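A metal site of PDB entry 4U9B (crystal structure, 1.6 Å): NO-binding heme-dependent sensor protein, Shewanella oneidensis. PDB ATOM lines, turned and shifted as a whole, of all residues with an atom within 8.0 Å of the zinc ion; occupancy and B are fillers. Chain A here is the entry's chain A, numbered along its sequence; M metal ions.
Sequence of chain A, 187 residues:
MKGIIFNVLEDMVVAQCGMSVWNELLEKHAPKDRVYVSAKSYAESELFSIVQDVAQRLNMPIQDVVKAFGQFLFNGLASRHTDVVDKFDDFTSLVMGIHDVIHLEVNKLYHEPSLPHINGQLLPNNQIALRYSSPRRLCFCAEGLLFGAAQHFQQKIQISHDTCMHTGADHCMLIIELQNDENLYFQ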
ATOM      1  N   GLN A  63      -9.051 -29.404 -21.551  1.00  0.00           N
ATOM      2  CA  GLN A  63      -9.077 -29.646 -20.118  1.00  0.00           C
ATOM      3  C   GLN A  63     -10.423 -30.192 -19.639  1.00  0.00           C
ATOM      4  O   GLN A  63     -10.482 -30.906 -18.643  1.00  0.00           O
ATOM      5  CB  GLN A  63      -8.731 -28.355 -19.360  1.00  0.00           C
ATOM      6  CG  GLN A  63      -7.313 -27.848 -19.633  1.00  0.00           C
ATOM      7  CD  GLN A  63      -6.244 -28.887 -19.315  1.00  0.00           C
ATOM      8  OE1 GLN A  63      -6.452 -29.774 -18.497  1.00  0.00           O
ATOM      9  NE2 GLN A  63      -5.103 -28.782 -19.989  1.00  0.00           N
ATOM     10  N   TYR A 132      -1.325 -30.183  -5.863  1.00  0.00           N
ATOM     11  CA  TYR A 132      -0.983 -31.010  -7.014  1.00  0.00           C
ATOM     12  C   TYR A 132       0.190 -30.390  -7.772  1.00  0.00           C
ATOM     13  O   TYR A 132       0.206 -29.185  -8.035  1.00  0.00           O
ATOM     14  CB  TYR A 132      -2.187 -31.169  -7.944  1.00  0.00           C
ATOM     15  CG  TYR A 132      -1.863 -31.839  -9.260  1.00  0.00           C
ATOM     16  CD1 TYR A 132      -1.429 -31.098 -10.349  1.00  0.00           C
ATOM     17  CD2 TYR A 132      -1.995 -33.207  -9.409  1.00  0.00           C
ATOM     18  CE1 TYR A 132      -1.126 -31.707 -11.545  1.00  0.00           C
ATOM     19  CE2 TYR A 132      -1.694 -33.831 -10.614  1.00  0.00           C
ATOM     20  CZ  TYR A 132      -1.267 -33.070 -11.676  1.00  0.00           C
ATOM     21  OH  TYR A 132      -0.963 -33.672 -12.885  1.00  0.00           O
ATOM     22  N   ARG A 137       1.075 -31.984 -16.001  1.00  0.00           N
ATOM     23  CA  ARG A 137       0.088 -30.911 -15.881  1.00  0.00           C
ATOM     24  C   ARG A 137      -1.328 -31.435 -16.082  1.00  0.00           C
ATOM     25  O   ARG A 137      -2.125 -30.884 -16.859  1.00  0.00           O
ATOM     26  CB  ARG A 137       0.404 -29.789 -16.875  1.00  0.00           C
ATOM     27  CG  ARG A 137       1.832 -29.268 -16.746  1.00  0.00           C
ATOM     28  CD  ARG A 137       1.963 -27.806 -17.164  1.00  0.00           C
ATOM     29  NE  ARG A 137       1.182 -27.494 -18.357  1.00  0.00           N
ATOM     30  CZ  ARG A 137       0.851 -26.265 -18.739  1.00  0.00           C
ATOM     31  NH1 ARG A 137       1.212 -25.219 -18.007  1.00  0.00           N
ATOM     32  NH2 ARG A 137       0.145 -26.085 -19.846  1.00  0.00           N
ATOM     33  N   LEU A 138      -1.654 -32.493 -15.352  1.00  0.00           N
ATOM     34  CA  LEU A 138      -2.954 -33.148 -15.450  1.00  0.00           C
ATOM     35  C   LEU A 138      -3.847 -32.868 -14.250  1.00  0.00           C
ATOM     36  O   LEU A 138      -4.561 -33.749 -13.759  1.00  0.00           O
ATOM     37  CB  LEU A 138      -2.764 -34.661 -15.617  1.00  0.00           C
ATOM     38  CG  LEU A 138      -2.344 -35.123 -17.020  1.00  0.00           C
ATOM     39  CD1 LEU A 138      -1.824 -36.548 -16.968  1.00  0.00           C
ATOM     40  CD2 LEU A 138      -3.509 -35.017 -17.983  1.00  0.00           C
ATOM     41  N   CYS A 139      -3.828 -31.633 -13.775  1.00  0.00           N
ATOM     42  CA  CYS A 139      -4.623 -31.256 -12.599  1.00  0.00           C
ATOM     43  C   CYS A 139      -6.116 -31.432 -12.859  1.00  0.00           C
ATOM     44  O   CYS A 139      -6.871 -31.697 -11.928  1.00  0.00           O
ATOM     45  CB  CYS A 139      -4.325 -29.817 -12.197  1.00  0.00           C
ATOM     46  SG  CYS A 139      -4.651 -28.602 -13.485  1.00  0.00           S
ATOM     47  N   PHE A 140      -6.540 -31.289 -14.104  1.00  0.00           N
ATOM     48  CA  PHE A 140      -7.954 -31.447 -14.423  1.00  0.00           C
ATOM     49  C   PHE A 140      -8.336 -32.917 -14.387  1.00  0.00           C
ATOM     50  O   PHE A 140      -9.494 -33.260 -14.098  1.00  0.00           O
ATOM     51  CB  PHE A 140      -8.288 -30.820 -15.777  1.00  0.00           C
ATOM     52  CG  PHE A 140      -8.643 -29.362 -15.701  1.00  0.00           C
ATOM     53  CD1 PHE A 140      -7.657 -28.403 -15.539  1.00  0.00           C
ATOM     54  CD2 PHE A 140      -9.958 -28.958 -15.796  1.00  0.00           C
ATOM     55  CE1 PHE A 140      -7.982 -27.071 -15.465  1.00  0.00           C
ATOM     56  CE2 PHE A 140     -10.291 -27.615 -15.717  1.00  0.00           C
ATOM     57  CZ  PHE A 140      -9.297 -26.667 -15.561  1.00  0.00           C
ATOM     58  N   ALA A 142      -6.896 -34.877 -12.199  1.00  0.00           N
ATOM     59  CA  ALA A 142      -6.968 -35.038 -10.747  1.00  0.00           C
ATOM     60  C   ALA A 142      -8.326 -34.600 -10.225  1.00  0.00           C
ATOM     61  O   ALA A 142      -8.924 -35.261  -9.381  1.00  0.00           O
ATOM     62  CB  ALA A 142      -5.850 -34.236 -10.071  1.00  0.00           C
ATOM     63  N   GLU A 143      -8.803 -33.466 -10.736  1.00  0.00           N
ATOM     64  CA  GLU A 143     -10.096 -32.932 -10.320  1.00  0.00           C
ATOM     65  C   GLU A 143     -11.180 -33.942 -10.689  1.00  0.00           C
ATOM     66  O   GLU A 143     -12.050 -34.252  -9.875  1.00  0.00           O
ATOM     67  CB  GLU A 143     -10.362 -31.572 -10.983  1.00  0.00           C
ATOM     68  CG  GLU A 143     -11.589 -30.857 -10.436  1.00  0.00           C
ATOM     69  CD  GLU A 143     -11.745 -29.439 -10.944  1.00  0.00           C
ATOM     70  OE1 GLU A 143     -10.736 -28.704 -11.053  1.00  0.00           O
ATOM     71  OE2 GLU A 143     -12.890 -29.046 -11.232  1.00  0.00           O
ATOM     72  N   HIS A 161     -10.380 -24.510  -7.391  1.00  0.00           N
ATOM     73  CA  HIS A 161      -9.102 -24.764  -8.034  1.00  0.00           C
ATOM     74  C   HIS A 161      -8.517 -23.412  -8.423  1.00  0.00           C
ATOM     75  O   HIS A 161      -8.367 -23.090  -9.601  1.00  0.00           O
ATOM     76  CB  HIS A 161      -9.347 -25.681  -9.246  1.00  0.00           C
ATOM     77  CG  HIS A 161      -8.098 -26.176  -9.924  1.00  0.00           C
ATOM     78  ND1 HIS A 161      -8.101 -27.280 -10.745  1.00  0.00           N
ATOM     79  CD2 HIS A 161      -6.824 -25.715  -9.913  1.00  0.00           C
ATOM     80  CE1 HIS A 161      -6.890 -27.481 -11.218  1.00  0.00           C
ATOM     81  NE2 HIS A 161      -6.094 -26.547 -10.732  1.00  0.00           N
ATOM     82  N   ASP A 162      -8.174 -22.615  -7.408  1.00  0.00           N
ATOM     83  CA  ASP A 162      -7.901 -21.188  -7.591  1.00  0.00           C
ATOM     84  C   ASP A 162      -6.407 -20.864  -7.766  1.00  0.00           C
ATOM     85  O   ASP A 162      -6.046 -19.732  -8.087  1.00  0.00           O
ATOM     86  CB  ASP A 162      -8.457 -20.387  -6.414  1.00  0.00           C
ATOM     87  CG  ASP A 162      -9.965 -20.444  -6.329  1.00  0.00           C
ATOM     88  OD1 ASP A 162     -10.634 -20.550  -7.388  1.00  0.00           O
ATOM     89  OD2 ASP A 162     -10.505 -20.379  -5.207  1.00  0.00           O
ATOM     90  N   THR A 163      -5.552 -21.853  -7.518  1.00  0.00           N
ATOM     91  CA  THR A 163      -4.157 -21.787  -7.930  1.00  0.00           C
ATOM     92  C   THR A 163      -3.963 -22.913  -8.941  1.00  0.00           C
ATOM     93  O   THR A 163      -4.386 -24.040  -8.692  1.00  0.00           O
ATOM     94  CB  THR A 163      -3.176 -21.959  -6.752  1.00  0.00           C
ATOM     95  OG1 THR A 163      -3.469 -20.984  -5.737  1.00  0.00           O
ATOM     96  CG2 THR A 163      -1.736 -21.792  -7.214  1.00  0.00           C
ATOM     97  N   CYS A 164      -3.346 -22.598 -10.075  1.00  0.00           N
ATOM     98  CA  CYS A 164      -3.218 -23.580 -11.147  1.00  0.00           C
ATOM     99  C   CYS A 164      -1.961 -23.395 -11.990  1.00  0.00           C
ATOM    100  O   CYS A 164      -1.585 -22.278 -12.335  1.00  0.00           O
ATOM    101  CB  CYS A 164      -4.452 -23.527 -12.061  1.00  0.00           C
ATOM    102  SG  CYS A 164      -4.490 -24.834 -13.305  1.00  0.00           S
ATOM    103  N   MET A 165      -1.337 -24.519 -12.319  1.00  0.00           N
ATOM    104  CA  MET A 165      -0.134 -24.533 -13.150  1.00  0.00           C
ATOM    105  C   MET A 165      -0.387 -23.971 -14.543  1.00  0.00           C
ATOM    106  O   MET A 165       0.514 -23.418 -15.179  1.00  0.00           O
ATOM    107  CB  MET A 165       0.410 -25.947 -13.268  1.00  0.00           C
ATOM    108  CG  MET A 165       0.828 -26.579 -11.955  1.00  0.00           C
ATOM    109  SD  MET A 165       1.441 -28.269 -12.145  1.00  0.00           S
ATOM    110  CE  MET A 165       3.026 -27.951 -12.914  1.00  0.00           C
ATOM    111  N   HIS A 166      -1.622 -24.112 -15.023  1.00  0.00           N
ATOM    112  CA  HIS A 166      -1.951 -23.678 -16.375  1.00  0.00           C
ATOM    113  C   HIS A 166      -1.940 -22.166 -16.522  1.00  0.00           C
ATOM    114  O   HIS A 166      -2.052 -21.659 -17.643  1.00  0.00           O
ATOM    115  CB  HIS A 166      -3.320 -24.234 -16.792  1.00  0.00           C
ATOM    116  CG  HIS A 166      -3.341 -25.723 -16.954  1.00  0.00           C
ATOM    117  ND1 HIS A 166      -2.601 -26.376 -17.910  1.00  0.00           N
ATOM    118  CD2 HIS A 166      -4.015 -26.684 -16.272  1.00  0.00           C
ATOM    119  CE1 HIS A 166      -2.816 -27.680 -17.820  1.00  0.00           C
ATOM    120  NE2 HIS A 166      -3.663 -27.890 -16.831  1.00  0.00           N
ATOM    121  N   THR A 167      -1.821 -21.449 -15.405  1.00  0.00           N
ATOM    122  CA  THR A 167      -1.735 -19.984 -15.454  1.00  0.00           C
ATOM    123  C   THR A 167      -0.341 -19.508 -15.063  1.00  0.00           C
ATOM    124  O   THR A 167      -0.096 -18.306 -15.006  1.00  0.00           O
ATOM    125  CB  THR A 167      -2.773 -19.320 -14.527  1.00  0.00           C
ATOM    126  OG1 THR A 167      -2.358 -19.429 -13.159  1.00  0.00           O
ATOM    127  CG2 THR A 167      -4.135 -19.970 -14.698  1.00  0.00           C
ATOM    128  N   ALA A 169       1.595 -20.920 -12.291  1.00  0.00           N
ATOM    129  CA  ALA A 169       2.002 -21.363 -10.949  1.00  0.00           C
ATOM    130  C   ALA A 169       2.811 -22.652 -11.039  1.00  0.00           C
ATOM    131  O   ALA A 169       2.743 -23.353 -12.049  1.00  0.00           O
ATOM    132  CB  ALA A 169       0.782 -21.552 -10.067  1.00  0.00           C
ATOM    133  N   HIS A 171       2.360 -25.114  -9.058  1.00  0.00           N
ATOM    134  CA  HIS A 171       1.516 -26.134  -8.445  1.00  0.00           C
ATOM    135  C   HIS A 171       0.055 -25.720  -8.572  1.00  0.00           C
ATOM    136  O   HIS A 171      -0.250 -24.566  -8.881  1.00  0.00           O
ATOM    137  CB  HIS A 171       1.863 -26.332  -6.974  1.00  0.00           C
ATOM    138  CG  HIS A 171       1.473 -25.175  -6.098  1.00  0.00           C
ATOM    139  ND1 HIS A 171       2.245 -24.048  -5.967  1.00  0.00           N
ATOM    140  CD2 HIS A 171       0.380 -24.972  -5.331  1.00  0.00           C
ATOM    141  CE1 HIS A 171       1.647 -23.201  -5.151  1.00  0.00           C
ATOM    142  NE2 HIS A 171       0.515 -23.731  -4.752  1.00  0.00           N
ATOM    143  N   CYS A 172      -0.842 -26.682  -8.340  1.00  0.00           N
ATOM    144  CA  CYS A 172      -2.267 -26.396  -8.222  1.00  0.00           C
ATOM    145  C   CYS A 172      -2.697 -26.621  -6.786  1.00  0.00           C
ATOM    146  O   CYS A 172      -2.125 -27.444  -6.074  1.00  0.00           O
ATOM    147  CB  CYS A 172      -3.088 -27.287  -9.151  1.00  0.00           C
ATOM    148  SG  CYS A 172      -2.595 -27.242 -10.874  1.00  0.00           S
ATOM    149  N   MET A 173      -3.727 -25.887  -6.382  1.00  0.00           N
ATOM    150  CA  MET A 173      -4.342 -26.055  -5.082  1.00  0.00           C
ATOM    151  C   MET A 173      -5.822 -26.323  -5.270  1.00  0.00           C
ATOM    152  O   MET A 173      -6.563 -25.454  -5.731  1.00  0.00           O
ATOM    153  CB  MET A 173      -4.122 -24.813  -4.211  1.00  0.00           C
ATOM    154  CG  MET A 173      -4.599 -24.967  -2.778  1.00  0.00           C
ATOM    155  SD  MET A 173      -3.857 -26.391  -1.932  1.00  0.00           S
ATOM    156  CE  MET A 173      -2.119 -26.029  -2.135  1.00  0.00           C
ATOM    157  N   LEU A 174      -6.236 -27.540  -4.940  1.00  0.00           N
ATOM    158  CA  LEU A 174      -7.629 -27.944  -5.036  1.00  0.00           C
ATOM    159  C   LEU A 174      -8.228 -28.036  -3.647  1.00  0.00           C
ATOM    160  O   LEU A 174      -7.873 -28.912  -2.860  1.00  0.00           O
ATOM    161  CB  LEU A 174      -7.749 -29.284  -5.764  1.00  0.00           C
ATOM    162  CG  LEU A 174      -7.575 -29.260  -7.284  1.00  0.00           C
ATOM    163  CD1 LEU A 174      -6.166 -28.886  -7.685  1.00  0.00           C
ATOM    164  CD2 LEU A 174      -7.953 -30.604  -7.887  1.00  0.00           C
HETATM  165 ZN    ZN M   1      -4.483 -26.743 -12.102  1.00  0.00          ZN
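N of Ala 169 lies close to O of Cys 164 (3.5 Å).
O of Tyr 132 is in hydrogen-bond range of N of Cys 172 (2.7 Å).
The side-chain sulfur (SG) of Cys 172 sits close to the backbone NH (N) of Met 165, 3.3 Å away.
The backbone carbonyl oxygen (O) of Cys 164 lies within hydrogen-bond range of the side-chain hydroxyl (OG1) of Thr 167, 3.1 Å away.
The backbone NH (N) of His 166 lies close to the side-chain sulfur (SG) of Cys 164 (3.4 Å).
SG of Cys 139 sits close to NE2 of His 166, at 3.6 Å.
The backbone carbonyl oxygen (O) of Met 165 sits at hydrogen-bond distance from the guanidinium group (NH1) of Arg 137 (3.4 Å).
The side-chain carboxylate of Glu 143 lies within hydrogen-bond range of a ring nitrogen (ND1) of His 161.
Merely in contact with the zinc ion: Met 165 (3.9 Å).
Within 4 Å of the zinc ion: Cys 139, His 161, Cys 164, Met 165 and Cys 172.
The nearest printed residue that does not touch the zinc ion is His 166 (4.2 Å).
The zinc ion is bound by a ring nitrogen (NE2) of His 161 (2.1 Å), the side-chain sulfur (SG) of Cys 164 (2.3 Å), the side-chain sulfur (SG) of Cys 172 (2.3 Å) and the side-chain sulfur (SG) of Cys 139 (2.3 Å).
The zinc ion has four donor atoms within binding distance.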
